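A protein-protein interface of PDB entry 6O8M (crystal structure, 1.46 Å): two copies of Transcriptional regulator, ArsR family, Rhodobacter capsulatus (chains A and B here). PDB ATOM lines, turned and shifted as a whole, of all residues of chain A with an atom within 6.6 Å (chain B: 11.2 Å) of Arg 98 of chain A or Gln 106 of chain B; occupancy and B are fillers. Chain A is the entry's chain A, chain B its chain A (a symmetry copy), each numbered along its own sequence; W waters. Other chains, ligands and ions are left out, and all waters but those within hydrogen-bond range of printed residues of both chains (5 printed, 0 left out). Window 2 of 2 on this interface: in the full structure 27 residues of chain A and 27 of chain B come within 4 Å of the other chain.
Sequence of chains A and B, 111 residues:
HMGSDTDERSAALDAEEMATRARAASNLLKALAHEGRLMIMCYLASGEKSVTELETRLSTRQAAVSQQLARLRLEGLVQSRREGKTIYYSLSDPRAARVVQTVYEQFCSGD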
ATOM      1  N   LEU A  91     -17.693   4.908 -15.698  1.00  0.00           N
ATOM      2  CA  LEU A  91     -17.761   6.357 -15.586  1.00  0.00           C
ATOM      3  C   LEU A  91     -18.778   6.906 -16.575  1.00  0.00           C
ATOM      4  O   LEU A  91     -18.901   6.427 -17.705  1.00  0.00           O
ATOM      5  CB  LEU A  91     -16.397   6.966 -15.870  1.00  0.00           C
ATOM      6  CG  LEU A  91     -15.347   6.642 -14.827  1.00  0.00           C
ATOM      7  CD1 LEU A  91     -14.118   7.457 -15.057  1.00  0.00           C
ATOM      8  CD2 LEU A  91     -15.836   6.869 -13.407  1.00  0.00           C
ATOM      9  N   ASP A  93     -19.742  10.664 -16.491  1.00  0.00           N
ATOM     10  CA  ASP A  93     -19.508  12.082 -16.729  1.00  0.00           C
ATOM     11  C   ASP A  93     -18.115  12.224 -17.314  1.00  0.00           C
ATOM     12  O   ASP A  93     -17.129  11.949 -16.614  1.00  0.00           O
ATOM     13  CB  ASP A  93     -19.615  12.831 -15.397  1.00  0.00           C
ATOM     14  CG  ASP A  93     -19.455  14.339 -15.530  1.00  0.00           C
ATOM     15  OD1 ASP A  93     -18.710  14.795 -16.411  1.00  0.00           O
ATOM     16  OD2 ASP A  93     -20.055  15.073 -14.717  1.00  0.00           O
ATOM     17  N   PRO A  94     -17.972  12.655 -18.569  1.00  0.00           N
ATOM     18  CA  PRO A  94     -16.628  12.705 -19.167  1.00  0.00           C
ATOM     19  C   PRO A  94     -15.723  13.752 -18.545  1.00  0.00           C
ATOM     20  O   PRO A  94     -14.495  13.597 -18.600  1.00  0.00           O
ATOM     21  CB  PRO A  94     -16.902  13.011 -20.647  1.00  0.00           C
ATOM     22  CG  PRO A  94     -18.238  13.741 -20.616  1.00  0.00           C
ATOM     23  CD  PRO A  94     -19.025  13.050 -19.519  1.00  0.00           C
ATOM     24  N   ARG A  95     -16.279  14.816 -17.968  1.00  0.00           N
ATOM     25  CA  ARG A  95     -15.429  15.782 -17.285  1.00  0.00           C
ATOM     26  C   ARG A  95     -14.771  15.125 -16.084  1.00  0.00           C
ATOM     27  O   ARG A  95     -13.560  15.254 -15.862  1.00  0.00           O
ATOM     28  CB  ARG A  95     -16.249  16.977 -16.806  1.00  0.00           C
ATOM     29  CG  ARG A  95     -16.956  17.750 -17.880  1.00  0.00           C
ATOM     30  CD  ARG A  95     -17.936  18.749 -17.264  1.00  0.00           C
ATOM     31  NE  ARG A  95     -18.960  18.082 -16.456  1.00  0.00           N
ATOM     32  CZ  ARG A  95     -19.954  18.708 -15.840  1.00  0.00           C
ATOM     33  NH1 ARG A  95     -20.083  20.022 -15.940  1.00  0.00           N
ATOM     34  NH2 ARG A  95     -20.822  18.007 -15.127  1.00  0.00           N
ATOM     35  N   ALA A  96     -15.572  14.406 -15.294  1.00  0.00           N
ATOM     36  CA  ALA A  96     -15.048  13.719 -14.127  1.00  0.00           C
ATOM     37  C   ALA A  96     -14.068  12.641 -14.537  1.00  0.00           C
ATOM     38  O   ALA A  96     -13.044  12.446 -13.877  1.00  0.00           O
ATOM     39  CB  ALA A  96     -16.199  13.124 -13.311  1.00  0.00           C
ATOM     40  N   ALA A  97     -14.348  11.945 -15.644  1.00  0.00           N
ATOM     41  CA  ALA A  97     -13.434  10.908 -16.097  1.00  0.00           C
ATOM     42  C   ALA A  97     -12.050  11.493 -16.342  1.00  0.00           C
ATOM     43  O   ALA A  97     -11.040  10.923 -15.921  1.00  0.00           O
ATOM     44  CB  ALA A  97     -13.971  10.245 -17.364  1.00  0.00           C
ATOM     45  N   ARG A  98     -11.989  12.641 -17.026  1.00  0.00           N
ATOM     46  CA  ARG A  98     -10.693  13.210 -17.361  1.00  0.00           C
ATOM     47  C   ARG A  98      -9.997  13.731 -16.117  1.00  0.00           C
ATOM     48  O   ARG A  98      -8.790  13.545 -15.956  1.00  0.00           O
ATOM     49  CB  ARG A  98     -10.855  14.312 -18.400  1.00  0.00           C
ATOM     50  CG  ARG A  98     -11.258  13.790 -19.793  1.00  0.00           C
ATOM     51  CD  ARG A  98     -10.254  12.807 -20.393  1.00  0.00           C
ATOM     52  NE  ARG A  98      -8.957  13.419 -20.657  1.00  0.00           N
ATOM     53  CZ  ARG A  98      -8.700  14.242 -21.675  1.00  0.00           C
ATOM     54  NH1 ARG A  98      -9.657  14.563 -22.544  1.00  0.00           N
ATOM     55  NH2 ARG A  98      -7.485  14.758 -21.821  1.00  0.00           N
ATOM     56  N   VAL A  99     -10.749  14.349 -15.209  1.00  0.00           N
ATOM     57  CA  VAL A  99     -10.163  14.804 -13.948  1.00  0.00           C
ATOM     58  C   VAL A  99      -9.557  13.627 -13.192  1.00  0.00           C
ATOM     59  O   VAL A  99      -8.411  13.687 -12.729  1.00  0.00           O
ATOM     60  CB  VAL A  99     -11.203  15.546 -13.095  1.00  0.00           C
ATOM     61  CG1 VAL A  99     -10.644  15.808 -11.722  1.00  0.00           C
ATOM     62  CG2 VAL A  99     -11.597  16.878 -13.771  1.00  0.00           C
ATOM     63  N   VAL A 100     -10.308  12.525 -13.082  1.00  0.00           N
ATOM     64  CA  VAL A 100      -9.816  11.364 -12.342  1.00  0.00           C
ATOM     65  C   VAL A 100      -8.622  10.743 -13.050  1.00  0.00           C
ATOM     66  O   VAL A 100      -7.670  10.303 -12.407  1.00  0.00           O
ATOM     67  CB  VAL A 100     -10.940  10.347 -12.123  1.00  0.00           C
ATOM     68  CG1 VAL A 100     -10.385   9.051 -11.558  1.00  0.00           C
ATOM     69  CG2 VAL A 100     -11.973  10.945 -11.180  1.00  0.00           C
ATOM     70  N   GLN A 101      -8.639  10.712 -14.380  1.00  0.00           N
ATOM     71  CA  GLN A 101      -7.488  10.177 -15.091  1.00  0.00           C
ATOM     72  C   GLN A 101      -6.242  10.998 -14.818  1.00  0.00           C
ATOM     73  O   GLN A 101      -5.151  10.445 -14.655  1.00  0.00           O
ATOM     74  CB  GLN A 101      -7.785  10.063 -16.578  1.00  0.00           C
ATOM     75  CG  GLN A 101      -8.634   8.834 -16.841  1.00  0.00           C
ATOM     76  CD  GLN A 101      -9.364   8.900 -18.110  1.00  0.00           C
ATOM     77  OE1 GLN A 101      -9.299   9.894 -18.834  1.00  0.00           O
ATOM     78  NE2 GLN A 101     -10.089   7.828 -18.414  1.00  0.00           N
ATOM     79  N   THR A 102      -6.388  12.320 -14.717  1.00  0.00           N
ATOM     80  CA  THR A 102      -5.235  13.140 -14.385  1.00  0.00           C
ATOM     81  C   THR A 102      -4.770  12.872 -12.963  1.00  0.00           C
ATOM     82  O   THR A 102      -3.568  12.725 -12.718  1.00  0.00           O
ATOM     83  CB  THR A 102      -5.573  14.614 -14.573  1.00  0.00           C
ATOM     84  OG1 THR A 102      -5.845  14.878 -15.950  1.00  0.00           O
ATOM     85  CG2 THR A 102      -4.413  15.491 -14.113  1.00  0.00           C
ATOM     86  N   VAL A 103      -5.707  12.784 -12.014  1.00  0.00           N
ATOM     87  CA  VAL A 103      -5.346  12.449 -10.641  1.00  0.00           C
ATOM     88  C   VAL A 103      -4.592  11.128 -10.595  1.00  0.00           C
ATOM     89  O   VAL A 103      -3.545  11.006  -9.946  1.00  0.00           O
ATOM     90  CB  VAL A 103      -6.607  12.401  -9.759  1.00  0.00           C
ATOM     91  CG1 VAL A 103      -6.257  11.869  -8.397  1.00  0.00           C
ATOM     92  CG2 VAL A 103      -7.243  13.781  -9.645  1.00  0.00           C
ATOM     93  N   LEU B  28      -5.242  16.701  -1.776  1.00  0.00           N
ATOM     94  CA  LEU B  28      -5.309  17.739  -2.796  1.00  0.00           C
ATOM     95  C   LEU B  28      -6.760  18.045  -3.124  1.00  0.00           C
ATOM     96  O   LEU B  28      -7.180  19.207  -3.174  1.00  0.00           O
ATOM     97  CB  LEU B  28      -4.557  17.322  -4.054  1.00  0.00           C
ATOM     98  CG  LEU B  28      -4.903  18.162  -5.285  1.00  0.00           C
ATOM     99  CD1 LEU B  28      -4.404  19.618  -5.176  1.00  0.00           C
ATOM    100  CD2 LEU B  28      -4.346  17.571  -6.559  1.00  0.00           C
ATOM    101  N   LEU B  29      -7.563  17.003  -3.328  1.00  0.00           N
ATOM    102  CA  LEU B  29      -8.934  17.241  -3.733  1.00  0.00           C
ATOM    103  C   LEU B  29      -9.709  17.974  -2.645  1.00  0.00           C
ATOM    104  O   LEU B  29     -10.526  18.845  -2.954  1.00  0.00           O
ATOM    105  CB  LEU B  29      -9.585  15.934  -4.172  1.00  0.00           C
ATOM    106  CG  LEU B  29      -8.930  15.346  -5.430  1.00  0.00           C
ATOM    107  CD1 LEU B  29      -9.381  13.916  -5.655  1.00  0.00           C
ATOM    108  CD2 LEU B  29      -9.253  16.206  -6.635  1.00  0.00           C
ATOM    109  N   LEU B  38     -10.635  26.847  -5.280  1.00  0.00           N
ATOM    110  CA  LEU B  38     -10.559  26.352  -6.644  1.00  0.00           C
ATOM    111  C   LEU B  38     -10.372  27.489  -7.636  1.00  0.00           C
ATOM    112  O   LEU B  38      -9.580  27.372  -8.574  1.00  0.00           O
ATOM    113  CB  LEU B  38     -11.820  25.568  -6.978  1.00  0.00           C
ATOM    114  CG  LEU B  38     -11.850  24.998  -8.392  1.00  0.00           C
ATOM    115  CD1 LEU B  38     -10.669  24.064  -8.626  1.00  0.00           C
ATOM    116  CD2 LEU B  38     -13.173  24.274  -8.641  1.00  0.00           C
ATOM    117  N   CYS B  42      -7.444  27.950 -10.280  1.00  0.00           N
ATOM    118  CA  CYS B  42      -7.700  28.061 -11.714  1.00  0.00           C
ATOM    119  C   CYS B  42      -7.015  29.281 -12.299  1.00  0.00           C
ATOM    120  O   CYS B  42      -6.489  29.231 -13.411  1.00  0.00           O
ATOM    121  CB  CYS B  42      -9.199  28.122 -11.971  1.00  0.00           C
ATOM    122  SG  CYS B  42     -10.006  26.501 -11.851  1.00  0.00           S
ATOM    123  N   ALA B  45      -3.425  28.568 -12.617  1.00  0.00           N
ATOM    124  CA  ALA B  45      -3.147  27.536 -13.607  1.00  0.00           C
ATOM    125  C   ALA B  45      -2.752  28.111 -14.946  1.00  0.00           C
ATOM    126  O   ALA B  45      -2.184  27.387 -15.765  1.00  0.00           O
ATOM    127  CB  ALA B  45      -4.364  26.634 -13.774  1.00  0.00           C
ATOM    128  N   ARG B  95       1.661  18.151  -9.717  1.00  0.00           N
ATOM    129  CA  ARG B  95       0.516  17.253  -9.787  1.00  0.00           C
ATOM    130  C   ARG B  95      -0.770  18.055  -9.681  1.00  0.00           C
ATOM    131  O   ARG B  95      -1.714  17.864 -10.458  1.00  0.00           O
ATOM    132  CB  ARG B  95       0.560  16.237  -8.648  1.00  0.00           C
ATOM    133  CG  ARG B  95       1.768  15.348  -8.619  1.00  0.00           C
ATOM    134  CD  ARG B  95       1.821  14.562  -7.308  1.00  0.00           C
ATOM    135  NE  ARG B  95       1.898  15.447  -6.143  1.00  0.00           N
ATOM    136  CZ  ARG B  95       1.993  15.029  -4.888  1.00  0.00           C
ATOM    137  NH1 ARG B  95       2.040  13.734  -4.616  1.00  0.00           N
ATOM    138  NH2 ARG B  95       2.048  15.917  -3.908  1.00  0.00           N
ATOM    139  N   ALA B  96      -0.815  18.968  -8.709  1.00  0.00           N
ATOM    140  CA  ALA B  96      -1.988  19.805  -8.525  1.00  0.00           C
ATOM    141  C   ALA B  96      -2.195  20.705  -9.724  1.00  0.00           C
ATOM    142  O   ALA B  96      -3.333  20.926 -10.149  1.00  0.00           O
ATOM    143  CB  ALA B  96      -1.844  20.631  -7.244  1.00  0.00           C
ATOM    144  N   ALA B  97      -1.103  21.214 -10.306  1.00  0.00           N
ATOM    145  CA  ALA B  97      -1.240  22.072 -11.473  1.00  0.00           C
ATOM    146  C   ALA B  97      -1.970  21.337 -12.587  1.00  0.00           C
ATOM    147  O   ALA B  97      -2.882  21.884 -13.213  1.00  0.00           O
ATOM    148  CB  ALA B  97       0.135  22.542 -11.947  1.00  0.00           C
ATOM    149  N   ARG B  98      -1.578  20.084 -12.848  1.00  0.00           N
ATOM    150  CA  ARG B  98      -2.183  19.356 -13.952  1.00  0.00           C
ATOM    151  C   ARG B  98      -3.626  19.006 -13.639  1.00  0.00           C
ATOM    152  O   ARG B  98      -4.493  19.115 -14.508  1.00  0.00           O
ATOM    153  CB  ARG B  98      -1.371  18.105 -14.264  1.00  0.00           C
ATOM    154  CG  ARG B  98       0.004  18.402 -14.892  1.00  0.00           C
ATOM    155  CD  ARG B  98      -0.080  19.173 -16.209  1.00  0.00           C
ATOM    156  NE  ARG B  98      -0.743  18.416 -17.264  1.00  0.00           N
ATOM    157  CZ  ARG B  98      -0.188  17.406 -17.935  1.00  0.00           C
ATOM    158  NH1 ARG B  98       1.058  17.019 -17.667  1.00  0.00           N
ATOM    159  NH2 ARG B  98      -0.884  16.770 -18.871  1.00  0.00           N
ATOM    160  N   VAL B  99      -3.907  18.627 -12.395  1.00  0.00           N
ATOM    161  CA  VAL B  99      -5.290  18.356 -12.000  1.00  0.00           C
ATOM    162  C   VAL B  99      -6.154  19.591 -12.217  1.00  0.00           C
ATOM    163  O   VAL B  99      -7.238  19.517 -12.810  1.00  0.00           O
ATOM    164  CB  VAL B  99      -5.359  17.868 -10.544  1.00  0.00           C
ATOM    165  CG1 VAL B  99      -6.794  17.808 -10.094  1.00  0.00           C
ATOM    166  CG2 VAL B  99      -4.702  16.476 -10.414  1.00  0.00           C
ATOM    167  N   VAL B 100      -5.674  20.755 -11.766  1.00  0.00           N
ATOM    168  CA  VAL B 100      -6.455  21.984 -11.901  1.00  0.00           C
ATOM    169  C   VAL B 100      -6.605  22.365 -13.367  1.00  0.00           C
ATOM    170  O   VAL B 100      -7.663  22.828 -13.789  1.00  0.00           O
ATOM    171  CB  VAL B 100      -5.832  23.116 -11.081  1.00  0.00           C
ATOM    172  CG1 VAL B 100      -6.506  24.439 -11.396  1.00  0.00           C
ATOM    173  CG2 VAL B 100      -5.962  22.785  -9.601  1.00  0.00           C
ATOM    174  N   GLN B 101      -5.564  22.159 -14.169  1.00  0.00           N
ATOM    175  CA  GLN B 101      -5.692  22.459 -15.587  1.00  0.00           C
ATOM    176  C   GLN B 101      -6.757  21.596 -16.237  1.00  0.00           C
ATOM    177  O   GLN B 101      -7.521  22.074 -17.080  1.00  0.00           O
ATOM    178  CB  GLN B 101      -4.347  22.332 -16.283  1.00  0.00           C
ATOM    179  CG  GLN B 101      -3.504  23.562 -16.005  1.00  0.00           C
ATOM    180  CD  GLN B 101      -2.070  23.334 -16.203  1.00  0.00           C
ATOM    181  OE1 GLN B 101      -1.637  22.225 -16.516  1.00  0.00           O
ATOM    182  NE2 GLN B 101      -1.288  24.393 -16.018  1.00  0.00           N
ATOM    183  N   THR B 102      -6.856  20.331 -15.828  1.00  0.00           N
ATOM    184  CA  THR B 102      -7.907  19.487 -16.371  1.00  0.00           C
ATOM    185  C   THR B 102      -9.276  19.963 -15.912  1.00  0.00           C
ATOM    186  O   THR B 102     -10.208  20.049 -16.718  1.00  0.00           O
ATOM    187  CB  THR B 102      -7.676  18.038 -15.962  1.00  0.00           C
ATOM    188  OG1 THR B 102      -6.462  17.557 -16.544  1.00  0.00           O
ATOM    189  CG2 THR B 102      -8.836  17.161 -16.422  1.00  0.00           C
ATOM    190  N   VAL B 103      -9.413  20.299 -14.626  1.00  0.00           N
ATOM    191  CA  VAL B 103     -10.673  20.840 -14.129  1.00  0.00           C
ATOM    192  C   VAL B 103     -11.069  22.079 -14.918  1.00  0.00           C
ATOM    193  O   VAL B 103     -12.219  22.224 -15.354  1.00  0.00           O
ATOM    194  CB  VAL B 103     -10.558  21.153 -12.625  1.00  0.00           C
ATOM    195  CG1 VAL B 103     -11.785  21.886 -12.161  1.00  0.00           C
ATOM    196  CG2 VAL B 103     -10.364  19.875 -11.818  1.00  0.00           C
ATOM    197  N   TYR B 104     -10.124  22.999 -15.089  1.00  0.00           N
ATOM    198  CA  TYR B 104     -10.402  24.266 -15.757  1.00  0.00           C
ATOM    199  C   TYR B 104     -10.833  24.037 -17.196  1.00  0.00           C
ATOM    200  O   TYR B 104     -11.815  24.625 -17.665  1.00  0.00           O
ATOM    201  CB  TYR B 104      -9.128  25.084 -15.685  1.00  0.00           C
ATOM    202  CG  TYR B 104      -9.184  26.561 -16.045  1.00  0.00           C
ATOM    203  CD1 TYR B 104     -10.098  27.425 -15.457  1.00  0.00           C
ATOM    204  CD2 TYR B 104      -8.263  27.098 -16.937  1.00  0.00           C
ATOM    205  CE1 TYR B 104     -10.089  28.788 -15.756  1.00  0.00           C
ATOM    206  CE2 TYR B 104      -8.259  28.454 -17.256  1.00  0.00           C
ATOM    207  CZ  TYR B 104      -9.176  29.292 -16.662  1.00  0.00           C
ATOM    208  OH  TYR B 104      -9.147  30.639 -16.988  1.00  0.00           O
ATOM    209  N   GLU B 105     -10.112  23.171 -17.911  1.00  0.00           N
ATOM    210  CA  GLU B 105     -10.468  22.885 -19.292  1.00  0.00           C
ATOM    211  C   GLU B 105     -11.819  22.198 -19.382  1.00  0.00           C
ATOM    212  O   GLU B 105     -12.662  22.574 -20.203  1.00  0.00           O
ATOM    213  CB  GLU B 105      -9.407  22.010 -19.934  1.00  0.00           C
ATOM    214  CG  GLU B 105      -9.720  21.594 -21.350  1.00  0.00           C
ATOM    215  CD  GLU B 105      -8.495  21.040 -22.036  1.00  0.00           C
ATOM    216  OE1 GLU B 105      -7.712  21.842 -22.579  1.00  0.00           O
ATOM    217  OE2 GLU B 105      -8.279  19.808 -21.994  1.00  0.00           O
ATOM    218  N   GLN B 106     -12.040  21.188 -18.546  1.00  0.00           N
ATOM    219  CA  GLN B 106     -13.270  20.414 -18.643  1.00  0.00           C
ATOM    220  C   GLN B 106     -14.474  21.233 -18.225  1.00  0.00           C
ATOM    221  O   GLN B 106     -15.514  21.196 -18.884  1.00  0.00           O
ATOM    222  CB  GLN B 106     -13.173  19.160 -17.778  1.00  0.00           C
ATOM    223  CG  GLN B 106     -12.178  18.139 -18.302  1.00  0.00           C
ATOM    224  CD  GLN B 106     -12.623  17.538 -19.608  1.00  0.00           C
ATOM    225  OE1 GLN B 106     -13.821  17.362 -19.840  1.00  0.00           O
ATOM    226  NE2 GLN B 106     -11.668  17.240 -20.481  1.00  0.00           N
ATOM    227  N   PHE B 107     -14.362  21.977 -17.128  1.00  0.00           N
ATOM    228  CA  PHE B 107     -15.523  22.675 -16.602  1.00  0.00           C
ATOM    229  C   PHE B 107     -15.749  24.031 -17.240  1.00  0.00           C
ATOM    230  O   PHE B 107     -16.865  24.556 -17.146  1.00  0.00           O
ATOM    231  CB  PHE B 107     -15.467  22.731 -15.079  1.00  0.00           C
ATOM    232  CG  PHE B 107     -15.844  21.422 -14.463  1.00  0.00           C
ATOM    233  CD1 PHE B 107     -17.156  21.154 -14.153  1.00  0.00           C
ATOM    234  CD2 PHE B 107     -14.901  20.427 -14.286  1.00  0.00           C
ATOM    235  CE1 PHE B 107     -17.513  19.939 -13.631  1.00  0.00           C
ATOM    236  CE2 PHE B 107     -15.264  19.194 -13.777  1.00  0.00           C
ATOM    237  CZ  PHE B 107     -16.565  18.959 -13.441  1.00  0.00           C
ATOM    238  N   CYS B 108     -14.758  24.602 -17.913  1.00  0.00           N
ATOM    239  CA  CYS B 108     -15.050  25.830 -18.640  1.00  0.00           C
ATOM    240  C   CYS B 108     -15.553  25.549 -20.048  1.00  0.00           C
ATOM    241  O   CYS B 108     -15.895  26.492 -20.767  1.00  0.00           O
ATOM    242  CB  CYS B 108     -13.831  26.745 -18.776  1.00  0.00           C
ATOM    243  SG  CYS B 108     -12.959  27.266 -17.329  1.00  0.00           S
ATOM    244  N   SER B 109     -15.539  24.289 -20.488  1.00  0.00           N
ATOM    245  CA  SER B 109     -16.021  23.960 -21.818  1.00  0.00           C
ATOM    246  C   SER B 109     -17.538  23.895 -21.795  1.00  0.00           C
ATOM    247  O   SER B 109     -18.130  23.292 -20.894  1.00  0.00           O
ATOM    248  CB  SER B 109     -15.442  22.628 -22.289  1.00  0.00           C
ATOM    249  OG  SER B 109     -14.037  22.718 -22.471  1.00  0.00           O
ATOM    250  N   GLY B 110     -18.127  24.519 -22.783  1.00  0.00           N
ATOM    251  CA  GLY B 110     -19.562  24.511 -23.020  1.00  0.00           C
ATOM    252  C   GLY B 110     -19.985  23.209 -23.658  1.00  0.00           C
ATOM    253  O   GLY B 110     -19.175  22.357 -23.971  1.00  0.00           O
ATOM    254  N   ASP B 111     -21.289  23.069 -23.799  1.00  0.00           N
ATOM    255  CA  ASP B 111     -21.755  21.809 -24.391  1.00  0.00           C
ATOM    256  C   ASP B 111     -22.401  22.133 -25.728  1.00  0.00           C
ATOM    257  O   ASP B 111     -21.703  22.772 -26.508  1.00  0.00           O
ATOM    258  CB  ASP B 111     -22.540  21.002 -23.370  1.00  0.00           C
ATOM    259  CG  ASP B 111     -21.775  19.713 -23.199  1.00  0.00           C
ATOM    260  OD1 ASP B 111     -21.556  19.048 -24.218  1.00  0.00           O
ATOM    261  OD2 ASP B 111     -21.341  19.445 -22.108  1.00  0.00           O
HETATM  262  O   HOH W   1      -6.565  16.935 -19.273  1.00  0.00           O
HETATM  263  O   HOH W   2     -12.069  14.874 -22.656  1.00  0.00           O
HETATM  264  O   HOH W   3     -18.962  22.455 -17.167  1.00  0.00           O
HETATM  265  O   HOH W   4      -3.617  15.011 -17.643  1.00  0.00           O
HETATM  266  O   HOH W   5      -7.616  17.674 -23.371  1.00  0.00           O
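Water W2 lies within hydrogen-bond range of the guanidinium group (NH1) of Arg 98 of chain A (2.4 Å) and the side-chain amide nitrogen (NE2) of Gln 106 of chain B (3.2 Å).
Water W5 lies within hydrogen-bond range of OE2 of Glu 105 of chain B (2.6 Å) and NH2 of Arg 98 of chain A (3.3 Å).
Water W1 lies within hydrogen-bond range of the side-chain hydroxyl (OG1) of Thr 102 of chain B (2.8 Å) and the guanidinium group (NH2) of Arg 98 of chain A (3.5 Å).
Water W4 lies within hydrogen-bond range of OG1 of Thr 102 of chain A (2.8 Å) and NH2 of Arg 98 of chain B (3.5 Å).
Water W3 lies within hydrogen-bond range of NH1 of Arg 95 of chain A (2.9 Å) and O of Phe 107 of chain B (3.0 Å).
Of the 22 printed residues of chain B, 6 touch a printed residue of chain A.
Hydrophobic or aromatic side chains of chain B within 4 Å of the printed part of chain A: Val 99, Val 103 and Phe 107.
The side-chain hydroxyl of Thr 102 of chain A is in hydrogen-bond range of the side-chain hydroxyl of Thr 102 of chain B, 2.8 Å away.
OD2 of Asp 93 of chain A lies within salt-bridge range of NH2 of Arg 95 of chain A (3.1 Å).
The backbone carbonyl oxygen of Arg 98 of chain A sits at hydrogen-bond distance from the side-chain hydroxyl of Thr 102 of chain A, at 3.2 Å.
O of Arg 98 of chain B is in hydrogen-bond range of OG1 of Thr 102 of chain B, at 3.2 Å.
Arg 98 of chain A touches Thr 102 of chain B, and with the chains exchanged Thr 102 of chain A touches Arg 98 of chain B.
Val 99 of chain A touches Thr 102 of chain B, and with the chains exchanged Thr 102 of chain A touches Val 99 of chain B.
Val 99 of chain A touches Val 103 of chain B, and with the chains exchanged Val 103 of chain A touches Val 99 of chain B.
Thr 102 of chain B touches its own counterpart, Thr 102 of chain A.
Positions printed for both chains: 95, 96, 97, 98, 99, 100, 101, 102 and 103.
Of the 10 pairs that touch across the chains among the printed residues, 7 have their exchanged pair printed and touching as well.
Gln 106 of chain B touches just these residues of chain A: Arg 95 and Arg 98.
No residue of chain B comes within 4 Å of Ala 97 of chain A.
No residue of chain B comes within 4 Å of Val 100 of chain A.
No residue of chain B comes within 4 Å of Gln 101 of chain A.
Thr 102 of chain A touches just these residues of chain B: Arg 98 (3.6 Å), Val 99 (3.6 Å) and Thr 102 (2.8 Å).
Printed residues of chain A within 4 Å of Val 103 of chain B: Val 99 (3.8 Å).
Of the printed residues of chain A, Thr 102 of chain B touches Arg 98 (3.6 Å), Val 99 (3.6 Å) and Thr 102 (2.8 Å).
Cys 42 of chain B touches none of the printed residues of chain A.
Gly 110 of chain B touches none of the printed residues of chain A.
The nearest residue of chain B that does not touch Arg 98 of chain A is Glu 105 of chain B (5.1 Å).
The nearest residue of chain A that does not touch Gln 106 of chain B is Pro 94 of chain A (4.02 Å).
The nearest printed residue of chain B that does not touch Arg 95 of chain A is Thr 102 of chain B (5.1 Å).
Among the printed residues, pairs that only touch across the chains: Arg 95 of chain A with Gln 106 of chain B, Arg 95 of chain A with Phe 107 of chain B, Arg 98 of chain A with Thr 102 of chain B, Arg 98 of chain A with Gln 106 of chain B, Val 99 of chain A with Thr 102 of chain B, Val 99 of chain A with Val 103 of chain B, Thr 102 of chain A with Arg 98 of chain B, Thr 102 of chain A with Val 99 of chain B and Val 103 of chain A with Val 99 of chain B.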
